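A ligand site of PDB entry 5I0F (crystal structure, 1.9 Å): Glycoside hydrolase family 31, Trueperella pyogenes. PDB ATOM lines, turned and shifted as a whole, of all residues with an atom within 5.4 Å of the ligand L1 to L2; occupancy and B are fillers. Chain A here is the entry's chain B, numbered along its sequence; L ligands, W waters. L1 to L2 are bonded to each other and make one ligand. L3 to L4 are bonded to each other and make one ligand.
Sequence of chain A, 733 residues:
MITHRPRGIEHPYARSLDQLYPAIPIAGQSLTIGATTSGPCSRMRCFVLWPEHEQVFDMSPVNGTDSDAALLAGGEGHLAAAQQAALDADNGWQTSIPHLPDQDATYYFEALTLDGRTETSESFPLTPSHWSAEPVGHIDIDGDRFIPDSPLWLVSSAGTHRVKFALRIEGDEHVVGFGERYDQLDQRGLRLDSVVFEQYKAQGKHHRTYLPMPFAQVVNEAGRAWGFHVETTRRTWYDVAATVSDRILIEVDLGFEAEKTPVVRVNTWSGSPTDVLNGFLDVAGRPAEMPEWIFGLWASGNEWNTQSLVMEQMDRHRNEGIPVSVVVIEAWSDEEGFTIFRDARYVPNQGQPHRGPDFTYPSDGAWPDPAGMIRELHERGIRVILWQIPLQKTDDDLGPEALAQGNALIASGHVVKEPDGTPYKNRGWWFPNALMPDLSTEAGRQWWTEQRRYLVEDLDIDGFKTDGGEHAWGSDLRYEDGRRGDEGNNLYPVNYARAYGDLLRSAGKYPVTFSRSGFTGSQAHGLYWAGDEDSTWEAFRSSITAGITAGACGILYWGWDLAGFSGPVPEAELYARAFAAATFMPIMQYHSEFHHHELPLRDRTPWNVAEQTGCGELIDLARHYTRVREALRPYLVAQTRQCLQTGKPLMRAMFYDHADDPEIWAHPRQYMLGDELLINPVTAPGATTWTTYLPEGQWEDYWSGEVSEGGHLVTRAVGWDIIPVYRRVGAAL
O2 of LG4 L4 is in hydrogen-bond range of O4 of LIG L1, at 2.9 Å.
O of Phe 565 lies within hydrogen-bond range of N of Glu 593, at 2.9 Å. The side-chain amide nitrogen (ND2) of Asn 302 sits at hydrogen-bond distance from the side-chain carboxylate (OE1) of Glu 330 (2.8 Å). OD1 of Asp 467 is in salt-bridge range of NE of Arg 516, at 3.3 Å. The backbone NH (N) of Asn 302 is in hydrogen-bond range of the backbone carbonyl oxygen (O) of Ser 592, 3.0 Å away. The side-chain amino group of Lys 393 sits at hydrogen-bond distance from the backbone carbonyl oxygen of Glu 335 (2.9 Å). The guanidinium group of Arg 516 is in salt-bridge range of the side-chain carboxylate of Asp 532 (3.7 Å). The side-chain carboxylate (OE2) of Glu 330 lies within salt-bridge range of the side-chain amino group (NZ) of Lys 465. The side-chain carboxylate of Asp 467 is in hydrogen-bond range of the indole nitrogen of Trp 387 (2.9 Å).
OD2 of Asp 532 is in hydrogen-bond range of O2 of LG4 L4, 2.7 Å away. OE2 of Glu 335 is in hydrogen-bond range of O5 of LG2 L2 (2.7 Å). The side-chain carboxylate (OE1) of Glu 330 is in hydrogen-bond range of an oxygen (O3) of LIG L1 (2.6 Å). NE1 of Trp 430 lies within hydrogen-bond range of O1 of LG2 L2 (3.4 Å). An oxygen (O1) of LG4 L4 is in hydrogen-bond range of the side-chain carboxylate (OE2) of Glu 593. OD2 of Asp 467 is bonded to C6 of LIG L1, 1.4 Å away. The guanidinium group (NH1) of Arg 516 sits at hydrogen-bond distance from an oxygen (O1) of LIG L1 (2.9 Å). The side-chain amide nitrogen (ND2) of Asn 302 sits at hydrogen-bond distance from an oxygen (O4) of LG2 L2, 2.9 Å away. An oxygen (O3) of LG3 L3 is in hydrogen-bond range of the backbone carbonyl oxygen (O) of Phe 594, at 2.7 Å. NE2 of His 591 is in hydrogen-bond range of O2 of LIG L1, 2.9 Å away. The side-chain amino group of Lys 465 sits at hydrogen-bond distance from an oxygen (O2) of LIG L1 (3.3 Å). OD1 of Asp 532 is in hydrogen-bond range of O1 of LIG L1 (2.7 Å). NH1 of Arg 516 sits at hydrogen-bond distance from O3 of LG4 L4, 3.0 Å away.
Water W5 bridges an oxygen (O5) of LG2 L2 (2.6 Å) and the side-chain amide oxygen (OD1) of Asn 302 (2.8 Å). Water W6 bridges an oxygen (O2) of LG2 L2 (2.7 Å) and the indole nitrogen of Trp 430 (3.4 Å). Water W2 bridges an oxygen (O2) of LG2 L2 (2.7 Å) and the side-chain amino group of Lys 393 (2.8 Å). Water W1 bridges an oxygen (O1) of LG4 L4 and an oxygen (O1) of LG2 L2. Water W3 lies within hydrogen-bond range of an oxygen (O3) of LIG L1 (2.8 Å) and the backbone NH (N) of Phe 594 (2.9 Å).
Residues that only touch the ligand L1 to L2: Ala 331, Phe 338, Trp 387, Phe 431, Trp 529 and Phe 565. Hydrophobic or aromatic side chains that line the ligand L1 to L2: Ala 331, Phe 338, Trp 387, Trp 430, Phe 431, Trp 529, Phe 565 and His 591. 15 residues have an atom within 4 Å of the ligand L1 to L2: Asn 302, Glu 330, Ala 331, Glu 335, Phe 338, Trp 387, Trp 430, Phe 431, Lys 465, Asp 467, Arg 516, Trp 529, Asp 532, Phe 565 and His 591.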
ATOM      1  N   ASN A 302     -20.726 -18.801  -7.293  1.00  0.00           N
ATOM      2  CA  ASN A 302     -22.100 -19.134  -6.924  1.00  0.00           C
ATOM      3  C   ASN A 302     -22.288 -19.413  -5.419  1.00  0.00           C
ATOM      4  O   ASN A 302     -23.378 -19.189  -4.888  1.00  0.00           O
ATOM      5  CB  ASN A 302     -22.649 -20.289  -7.761  1.00  0.00           C
ATOM      6  CG  ASN A 302     -24.125 -20.536  -7.488  1.00  0.00           C
ATOM      7  OD1 ASN A 302     -24.488 -21.373  -6.628  1.00  0.00           O
ATOM      8  ND2 ASN A 302     -24.976 -19.782  -8.142  1.00  0.00           N
ATOM      9  N   GLU A 330     -24.884 -14.368  -7.267  1.00  0.00           N
ATOM     10  CA  GLU A 330     -25.882 -15.243  -7.868  1.00  0.00           C
ATOM     11  C   GLU A 330     -26.869 -15.754  -6.858  1.00  0.00           C
ATOM     12  O   GLU A 330     -28.087 -15.645  -7.080  1.00  0.00           O
ATOM     13  CB  GLU A 330     -25.195 -16.427  -8.589  1.00  0.00           C
ATOM     14  CG  GLU A 330     -24.343 -15.973  -9.732  1.00  0.00           C
ATOM     15  CD  GLU A 330     -24.033 -17.074 -10.729  1.00  0.00           C
ATOM     16  OE1 GLU A 330     -23.891 -18.266 -10.294  1.00  0.00           O
ATOM     17  OE2 GLU A 330     -23.920 -16.737 -11.932  1.00  0.00           O
ATOM     18  N   ALA A 331     -26.353 -16.290  -5.757  1.00  0.00           N
ATOM     19  CA  ALA A 331     -27.177 -16.837  -4.679  1.00  0.00           C
ATOM     20  C   ALA A 331     -27.426 -15.750  -3.628  1.00  0.00           C
ATOM     21  O   ALA A 331     -26.898 -15.806  -2.535  1.00  0.00           O
ATOM     22  CB  ALA A 331     -26.480 -18.047  -4.051  1.00  0.00           C
ATOM     23  N   GLU A 335     -34.437 -17.837  -3.458  1.00  0.00           N
ATOM     24  CA  GLU A 335     -34.369 -19.017  -4.339  1.00  0.00           C
ATOM     25  C   GLU A 335     -35.749 -19.576  -4.735  1.00  0.00           C
ATOM     26  O   GLU A 335     -35.859 -20.710  -5.212  1.00  0.00           O
ATOM     27  CB  GLU A 335     -33.498 -20.135  -3.738  1.00  0.00           C
ATOM     28  CG  GLU A 335     -32.030 -19.730  -3.568  1.00  0.00           C
ATOM     29  CD  GLU A 335     -31.284 -19.533  -4.897  1.00  0.00           C
ATOM     30  OE1 GLU A 335     -31.624 -20.200  -5.907  1.00  0.00           O
ATOM     31  OE2 GLU A 335     -30.336 -18.703  -4.925  1.00  0.00           O
ATOM     32  N   PHE A 338     -36.686 -14.947  -6.911  1.00  0.00           N
ATOM     33  CA  PHE A 338     -35.554 -14.143  -7.449  1.00  0.00           C
ATOM     34  C   PHE A 338     -35.832 -12.646  -7.489  1.00  0.00           C
ATOM     35  O   PHE A 338     -35.412 -11.931  -8.395  1.00  0.00           O
ATOM     36  CB  PHE A 338     -35.076 -14.739  -8.771  1.00  0.00           C
ATOM     37  CG  PHE A 338     -34.715 -16.172  -8.624  1.00  0.00           C
ATOM     38  CD1 PHE A 338     -33.479 -16.536  -8.113  1.00  0.00           C
ATOM     39  CD2 PHE A 338     -35.670 -17.178  -8.858  1.00  0.00           C
ATOM     40  CE1 PHE A 338     -33.154 -17.857  -7.878  1.00  0.00           C
ATOM     41  CE2 PHE A 338     -35.348 -18.523  -8.625  1.00  0.00           C
ATOM     42  CZ  PHE A 338     -34.092 -18.870  -8.138  1.00  0.00           C
ATOM     43  N   TRP A 387     -27.958 -11.788 -10.120  1.00  0.00           N
ATOM     44  CA  TRP A 387     -28.397 -12.824 -11.057  1.00  0.00           C
ATOM     45  C   TRP A 387     -29.911 -12.873 -11.199  1.00  0.00           C
ATOM     46  O   TRP A 387     -30.639 -12.645 -10.232  1.00  0.00           O
ATOM     47  CB  TRP A 387     -27.899 -14.164 -10.536  1.00  0.00           C
ATOM     48  CG  TRP A 387     -28.113 -15.400 -11.376  1.00  0.00           C
ATOM     49  CD1 TRP A 387     -27.217 -15.946 -12.245  1.00  0.00           C
ATOM     50  CD2 TRP A 387     -29.230 -16.291 -11.354  1.00  0.00           C
ATOM     51  NE1 TRP A 387     -27.714 -17.114 -12.762  1.00  0.00           N
ATOM     52  CE2 TRP A 387     -28.950 -17.338 -12.248  1.00  0.00           C
ATOM     53  CE3 TRP A 387     -30.441 -16.299 -10.668  1.00  0.00           C
ATOM     54  CZ2 TRP A 387     -29.846 -18.390 -12.492  1.00  0.00           C
ATOM     55  CZ3 TRP A 387     -31.323 -17.337 -10.892  1.00  0.00           C
ATOM     56  CH2 TRP A 387     -31.021 -18.377 -11.806  1.00  0.00           C
ATOM     57  N   LYS A 393     -40.723 -20.056 -11.078  1.00  0.00           N
ATOM     58  CA  LYS A 393     -40.939 -21.412 -10.565  1.00  0.00           C
ATOM     59  C   LYS A 393     -42.394 -21.609 -10.152  1.00  0.00           C
ATOM     60  O   LYS A 393     -43.058 -20.684  -9.717  1.00  0.00           O
ATOM     61  CB  LYS A 393     -40.059 -21.707  -9.361  1.00  0.00           C
ATOM     62  CG  LYS A 393     -38.569 -21.827  -9.621  1.00  0.00           C
ATOM     63  CD  LYS A 393     -37.833 -22.021  -8.295  1.00  0.00           C
ATOM     64  CE  LYS A 393     -36.407 -22.518  -8.492  1.00  0.00           C
ATOM     65  NZ  LYS A 393     -35.711 -22.828  -7.217  1.00  0.00           N
ATOM     66  N   TRP A 430     -33.669 -27.715 -16.822  1.00  0.00           N
ATOM     67  CA  TRP A 430     -33.353 -26.738 -15.748  1.00  0.00           C
ATOM     68  C   TRP A 430     -34.596 -25.893 -15.482  1.00  0.00           C
ATOM     69  O   TRP A 430     -35.178 -25.341 -16.418  1.00  0.00           O
ATOM     70  CB  TRP A 430     -32.219 -25.859 -16.250  1.00  0.00           C
ATOM     71  CG  TRP A 430     -31.496 -24.999 -15.246  1.00  0.00           C
ATOM     72  CD1 TRP A 430     -31.095 -25.341 -13.988  1.00  0.00           C
ATOM     73  CD2 TRP A 430     -31.014 -23.678 -15.487  1.00  0.00           C
ATOM     74  NE1 TRP A 430     -30.428 -24.292 -13.410  1.00  0.00           N
ATOM     75  CE2 TRP A 430     -30.359 -23.255 -14.306  1.00  0.00           C
ATOM     76  CE3 TRP A 430     -31.093 -22.799 -16.576  1.00  0.00           C
ATOM     77  CZ2 TRP A 430     -29.773 -21.992 -14.184  1.00  0.00           C
ATOM     78  CZ3 TRP A 430     -30.503 -21.544 -16.472  1.00  0.00           C
ATOM     79  CH2 TRP A 430     -29.850 -21.150 -15.280  1.00  0.00           C
ATOM     80  N   PHE A 431     -34.991 -25.784 -14.215  1.00  0.00           N
ATOM     81  CA  PHE A 431     -36.244 -25.116 -13.811  1.00  0.00           C
ATOM     82  C   PHE A 431     -37.419 -25.750 -14.568  1.00  0.00           C
ATOM     83  O   PHE A 431     -38.181 -25.065 -15.249  1.00  0.00           O
ATOM     84  CB  PHE A 431     -36.208 -23.589 -14.084  1.00  0.00           C
ATOM     85  CG  PHE A 431     -35.340 -22.798 -13.137  1.00  0.00           C
ATOM     86  CD1 PHE A 431     -33.954 -22.959 -13.117  1.00  0.00           C
ATOM     87  CD2 PHE A 431     -35.894 -21.826 -12.315  1.00  0.00           C
ATOM     88  CE1 PHE A 431     -33.145 -22.214 -12.255  1.00  0.00           C
ATOM     89  CE2 PHE A 431     -35.102 -21.063 -11.453  1.00  0.00           C
ATOM     90  CZ  PHE A 431     -33.725 -21.270 -11.405  1.00  0.00           C
ATOM     91  N   LYS A 465     -27.031 -10.037 -14.047  1.00  0.00           N
ATOM     92  CA  LYS A 465     -26.601 -11.203 -14.797  1.00  0.00           C
ATOM     93  C   LYS A 465     -27.850 -11.943 -15.262  1.00  0.00           C
ATOM     94  O   LYS A 465     -28.422 -12.753 -14.512  1.00  0.00           O
ATOM     95  CB  LYS A 465     -25.709 -12.116 -13.954  1.00  0.00           C
ATOM     96  CG  LYS A 465     -25.152 -13.300 -14.742  1.00  0.00           C
ATOM     97  CD  LYS A 465     -24.109 -14.068 -13.966  1.00  0.00           C
ATOM     98  CE  LYS A 465     -23.543 -15.191 -14.822  1.00  0.00           C
ATOM     99  NZ  LYS A 465     -22.445 -15.911 -14.118  1.00  0.00           N
ATOM    100  N   ASP A 467     -29.108 -14.518 -16.898  1.00  0.00           N
ATOM    101  CA  ASP A 467     -28.791 -15.889 -17.279  1.00  0.00           C
ATOM    102  C   ASP A 467     -30.008 -16.558 -17.944  1.00  0.00           C
ATOM    103  O   ASP A 467     -31.133 -16.082 -17.817  1.00  0.00           O
ATOM    104  CB  ASP A 467     -28.362 -16.646 -15.996  1.00  0.00           C
ATOM    105  CG  ASP A 467     -27.582 -17.923 -16.254  1.00  0.00           C
ATOM    106  OD1 ASP A 467     -27.258 -18.276 -17.393  1.00  0.00           O
ATOM    107  OD2 ASP A 467     -27.246 -18.592 -15.231  1.00  0.00           O
ATOM    108  N   GLY A 468     -29.769 -17.647 -18.641  1.00  0.00           N
ATOM    109  CA  GLY A 468     -30.823 -18.369 -19.364  1.00  0.00           C
ATOM    110  C   GLY A 468     -31.391 -17.636 -20.573  1.00  0.00           C
ATOM    111  O   GLY A 468     -30.687 -16.901 -21.247  1.00  0.00           O
ATOM    112  N   ARG A 516     -25.727 -14.914 -21.529  1.00  0.00           N
ATOM    113  CA  ARG A 516     -25.068 -15.955 -22.317  1.00  0.00           C
ATOM    114  C   ARG A 516     -25.800 -16.232 -23.624  1.00  0.00           C
ATOM    115  O   ARG A 516     -25.166 -16.693 -24.572  1.00  0.00           O
ATOM    116  CB  ARG A 516     -24.914 -17.274 -21.537  1.00  0.00           C
ATOM    117  CG  ARG A 516     -26.243 -17.937 -21.163  1.00  0.00           C
ATOM    118  CD  ARG A 516     -26.079 -19.165 -20.273  1.00  0.00           C
ATOM    119  NE  ARG A 516     -27.352 -19.887 -20.217  1.00  0.00           N
ATOM    120  CZ  ARG A 516     -27.622 -20.922 -19.418  1.00  0.00           C
ATOM    121  NH1 ARG A 516     -26.729 -21.370 -18.536  1.00  0.00           N
ATOM    122  NH2 ARG A 516     -28.789 -21.531 -19.494  1.00  0.00           N
ATOM    123  N   TRP A 529     -21.164 -13.372 -21.959  1.00  0.00           N
ATOM    124  CA  TRP A 529     -20.110 -14.306 -21.623  1.00  0.00           C
ATOM    125  C   TRP A 529     -20.387 -15.628 -22.321  1.00  0.00           C
ATOM    126  O   TRP A 529     -21.515 -15.891 -22.720  1.00  0.00           O
ATOM    127  CB  TRP A 529     -19.884 -14.438 -20.096  1.00  0.00           C
ATOM    128  CG  TRP A 529     -20.654 -15.525 -19.403  1.00  0.00           C
ATOM    129  CD1 TRP A 529     -20.161 -16.737 -19.015  1.00  0.00           C
ATOM    130  CD2 TRP A 529     -22.018 -15.494 -18.973  1.00  0.00           C
ATOM    131  NE1 TRP A 529     -21.147 -17.488 -18.428  1.00  0.00           N
ATOM    132  CE2 TRP A 529     -22.301 -16.742 -18.366  1.00  0.00           C
ATOM    133  CE3 TRP A 529     -23.039 -14.536 -19.021  1.00  0.00           C
ATOM    134  CZ2 TRP A 529     -23.549 -17.065 -17.836  1.00  0.00           C
ATOM    135  CZ3 TRP A 529     -24.286 -14.854 -18.504  1.00  0.00           C
ATOM    136  CH2 TRP A 529     -24.539 -16.120 -17.927  1.00  0.00           C
ATOM    137  N   GLY A 531     -20.693 -18.713 -21.497  1.00  0.00           N
ATOM    138  CA  GLY A 531     -21.483 -19.781 -20.872  1.00  0.00           C
ATOM    139  C   GLY A 531     -20.664 -20.775 -20.081  1.00  0.00           C
ATOM    140  O   GLY A 531     -19.601 -20.438 -19.517  1.00  0.00           O
ATOM    141  N   ASP A 532     -21.178 -22.004 -20.009  1.00  0.00           N
ATOM    142  CA  ASP A 532     -20.711 -22.986 -19.045  1.00  0.00           C
ATOM    143  C   ASP A 532     -19.683 -23.933 -19.634  1.00  0.00           C
ATOM    144  O   ASP A 532     -19.965 -24.589 -20.634  1.00  0.00           O
ATOM    145  CB  ASP A 532     -21.884 -23.835 -18.576  1.00  0.00           C
ATOM    146  CG  ASP A 532     -22.907 -23.056 -17.815  1.00  0.00           C
ATOM    147  OD1 ASP A 532     -22.623 -21.924 -17.370  1.00  0.00           O
ATOM    148  OD2 ASP A 532     -24.007 -23.620 -17.603  1.00  0.00           O
ATOM    149  N   ASP A 561     -15.711 -17.349 -18.373  1.00  0.00           N
ATOM    150  CA  ASP A 561     -15.274 -17.793 -17.040  1.00  0.00           C
ATOM    151  C   ASP A 561     -13.823 -18.260 -17.166  1.00  0.00           C
ATOM    152  O   ASP A 561     -13.564 -19.356 -17.654  1.00  0.00           O
ATOM    153  CB  ASP A 561     -16.105 -18.971 -16.569  1.00  0.00           C
ATOM    154  CG  ASP A 561     -17.596 -18.668 -16.452  1.00  0.00           C
ATOM    155  OD1 ASP A 561     -18.041 -17.489 -16.346  1.00  0.00           O
ATOM    156  OD2 ASP A 561     -18.330 -19.681 -16.471  1.00  0.00           O
ATOM    157  N   PHE A 565     -15.541 -22.862 -15.020  1.00  0.00           N
ATOM    158  CA  PHE A 565     -16.255 -22.716 -13.759  1.00  0.00           C
ATOM    159  C   PHE A 565     -16.672 -24.029 -13.093  1.00  0.00           C
ATOM    160  O   PHE A 565     -17.033 -23.996 -11.907  1.00  0.00           O
ATOM    161  CB  PHE A 565     -17.431 -21.733 -13.902  1.00  0.00           C
ATOM    162  CG  PHE A 565     -18.787 -22.358 -14.141  1.00  0.00           C
ATOM    163  CD1 PHE A 565     -19.006 -23.354 -15.072  1.00  0.00           C
ATOM    164  CD2 PHE A 565     -19.894 -21.831 -13.497  1.00  0.00           C
ATOM    165  CE1 PHE A 565     -20.279 -23.886 -15.284  1.00  0.00           C
ATOM    166  CE2 PHE A 565     -21.157 -22.327 -13.711  1.00  0.00           C
ATOM    167  CZ  PHE A 565     -21.357 -23.359 -14.610  1.00  0.00           C
ATOM    168  N   HIS A 591     -15.219 -17.112 -12.155  1.00  0.00           N
ATOM    169  CA  HIS A 591     -16.515 -17.615 -11.707  1.00  0.00           C
ATOM    170  C   HIS A 591     -16.406 -19.082 -11.299  1.00  0.00           C
ATOM    171  O   HIS A 591     -15.514 -19.798 -11.741  1.00  0.00           O
ATOM    172  CB  HIS A 591     -17.554 -17.408 -12.837  1.00  0.00           C
ATOM    173  CG  HIS A 591     -18.954 -17.838 -12.512  1.00  0.00           C
ATOM    174  ND1 HIS A 591     -19.578 -17.516 -11.336  1.00  0.00           N
ATOM    175  CD2 HIS A 591     -19.862 -18.516 -13.250  1.00  0.00           C
ATOM    176  CE1 HIS A 591     -20.792 -18.047 -11.323  1.00  0.00           C
ATOM    177  NE2 HIS A 591     -21.000 -18.647 -12.483  1.00  0.00           N
ATOM    178  N   SER A 592     -17.321 -19.527 -10.454  1.00  0.00           N
ATOM    179  CA  SER A 592     -17.411 -20.932 -10.067  1.00  0.00           C
ATOM    180  C   SER A 592     -18.850 -21.433  -9.934  1.00  0.00           C
ATOM    181  O   SER A 592     -19.741 -20.751  -9.400  1.00  0.00           O
ATOM    182  CB  SER A 592     -16.679 -21.175  -8.744  1.00  0.00           C
ATOM    183  OG  SER A 592     -17.201 -20.386  -7.681  1.00  0.00           O
ATOM    184  N   GLU A 593     -19.043 -22.647 -10.388  1.00  0.00           N
ATOM    185  CA  GLU A 593     -20.344 -23.307 -10.354  1.00  0.00           C
ATOM    186  C   GLU A 593     -20.717 -23.764  -8.944  1.00  0.00           C
ATOM    187  O   GLU A 593     -19.855 -24.121  -8.141  1.00  0.00           O
ATOM    188  CB  GLU A 593     -20.311 -24.516 -11.299  1.00  0.00           C
ATOM    189  CG  GLU A 593     -21.657 -25.204 -11.531  1.00  0.00           C
ATOM    190  CD  GLU A 593     -21.574 -26.309 -12.573  1.00  0.00           C
ATOM    191  OE1 GLU A 593     -20.593 -27.072 -12.550  1.00  0.00           O
ATOM    192  OE2 GLU A 593     -22.478 -26.417 -13.415  1.00  0.00           O
ATOM    193  N   PHE A 594     -22.021 -23.793  -8.673  1.00  0.00           N
ATOM    194  CA  PHE A 594     -22.627 -24.370  -7.473  1.00  0.00           C
ATOM    195  C   PHE A 594     -22.109 -25.787  -7.260  1.00  0.00           C
ATOM    196  O   PHE A 594     -22.023 -26.548  -8.211  1.00  0.00           O
ATOM    197  CB  PHE A 594     -24.153 -24.441  -7.631  1.00  0.00           C
ATOM    198  CG  PHE A 594     -24.886 -24.872  -6.390  1.00  0.00           C
ATOM    199  CD1 PHE A 594     -24.770 -24.166  -5.197  1.00  0.00           C
ATOM    200  CD2 PHE A 594     -25.749 -25.965  -6.431  1.00  0.00           C
ATOM    201  CE1 PHE A 594     -25.462 -24.563  -4.049  1.00  0.00           C
ATOM    202  CE2 PHE A 594     -26.448 -26.368  -5.293  1.00  0.00           C
ATOM    203  CZ  PHE A 594     -26.311 -25.660  -4.107  1.00  0.00           C
HETATM  204  C1  LIG L   1     -24.947 -19.808 -15.607  1.00  0.00           C
HETATM  205  C2  LIG L   1     -23.880 -20.019 -14.524  1.00  0.00           C
HETATM  206  C3  LIG L   1     -24.508 -19.786 -13.155  1.00  0.00           C
HETATM  207  C4  LIG L   1     -25.740 -20.681 -12.960  1.00  0.00           C
HETATM  208  C5  LIG L   1     -26.458 -20.274 -11.677  1.00  0.00           C
HETATM  209  C6  LIG L   1     -26.433 -19.784 -15.194  1.00  0.00           C
HETATM  210  O1  LIG L   1     -24.618 -20.164 -16.967  1.00  0.00           O
HETATM  211  O2  LIG L   1     -22.769 -19.140 -14.731  1.00  0.00           O
HETATM  212  O3  LIG L   1     -23.550 -20.042 -12.103  1.00  0.00           O
HETATM  213  O4  LIG L   1     -26.689 -20.629 -14.059  1.00  0.00           O
HETATM  214  O5  LIG L   1     -27.476 -21.224 -11.338  1.00  0.00           O
HETATM  215  C1  LG2 L   2     -27.367 -21.735 -10.005  1.00  0.00           C
HETATM  216  C2  LG2 L   2     -28.351 -22.901  -9.800  1.00  0.00           C
HETATM  217  C3  LG2 L   2     -29.790 -22.402  -9.685  1.00  0.00           C
HETATM  218  C4  LG2 L   2     -29.876 -21.284  -8.661  1.00  0.00           C
HETATM  219  C5  LG2 L   2     -28.912 -20.163  -9.018  1.00  0.00           C
HETATM  220  C6  LG2 L   2     -28.953 -19.005  -8.032  1.00  0.00           C
HETATM  221  O1  LG2 L   2     -28.258 -23.827 -10.881  1.00  0.00           O
HETATM  222  O2  LG2 L   2     -30.646 -23.496  -9.334  1.00  0.00           O
HETATM  223  O3  LG2 L   2     -31.233 -20.784  -8.614  1.00  0.00           O
HETATM  224  O4  LG2 L   2     -27.590 -20.694  -9.038  1.00  0.00           O
HETATM  225  O5  LG2 L   2     -28.517 -19.430  -6.752  1.00  0.00           O
HETATM  226  C1  LG3 L   3     -25.197 -30.133 -12.462  1.00  0.00           C
HETATM  227  C2  LG3 L   3     -23.951 -29.645 -11.715  1.00  0.00           C
HETATM  228  C3  LG3 L   3     -24.343 -28.697 -10.586  1.00  0.00           C
HETATM  229  C4  LG3 L   3     -25.202 -27.548 -11.107  1.00  0.00           C
HETATM  230  C5  LG3 L   3     -26.429 -28.139 -11.818  1.00  0.00           C
HETATM  231  C6  LG3 L   3     -27.428 -27.125 -12.397  1.00  0.00           C
HETATM  232  O1  LG3 L   3     -25.980 -30.955 -11.594  1.00  0.00           O
HETATM  233  O2  LG3 L   3     -23.236 -30.776 -11.193  1.00  0.00           O
HETATM  234  O3  LG3 L   3     -23.143 -28.217  -9.969  1.00  0.00           O
HETATM  235  O4  LG3 L   3     -25.627 -26.704 -10.032  1.00  0.00           O
HETATM  236  O5  LG3 L   3     -25.968 -29.000 -12.877  1.00  0.00           O
HETATM  237  O6  LG3 L   3     -26.795 -25.972 -12.996  1.00  0.00           O
HETATM  238  C1  LG4 L   4     -26.081 -26.260 -14.220  1.00  0.00           C
HETATM  239  C2  LG4 L   4     -25.304 -25.007 -14.624  1.00  0.00           C
HETATM  240  C3  LG4 L   4     -26.246 -23.933 -15.135  1.00  0.00           C
HETATM  241  C4  LG4 L   4     -27.066 -24.473 -16.298  1.00  0.00           C
HETATM  242  C5  LG4 L   4     -27.835 -25.692 -15.783  1.00  0.00           C
HETATM  243  C6  LG4 L   4     -28.721 -26.332 -16.832  1.00  0.00           C
HETATM  244  O1  LG4 L   4     -24.538 -24.541 -13.511  1.00  0.00           O
HETATM  245  O2  LG4 L   4     -25.483 -22.788 -15.565  1.00  0.00           O
HETATM  246  O3  LG4 L   4     -27.956 -23.462 -16.803  1.00  0.00           O
HETATM  247  O4  LG4 L   4     -26.924 -26.701 -15.285  1.00  0.00           O
HETATM  248  O5  LG4 L   4     -27.956 -27.013 -17.834  1.00  0.00           O
HETATM  249  O   HOH W   1     -25.571 -24.266 -11.150  1.00  0.00           O
HETATM  250  O   HOH W   2     -33.071 -23.354  -8.106  1.00  0.00           O
HETATM  251  O   HOH W   3     -23.687 -22.366 -10.519  1.00  0.00           O
HETATM  252  O   HOH W   4     -21.044 -19.779 -16.630  1.00  0.00           O
HETATM  253  O   HOH W   5     -27.191 -21.501  -5.893  1.00  0.00           O
HETATM  254  O   HOH W   6     -30.891 -25.910 -10.479  1.00  0.00           O
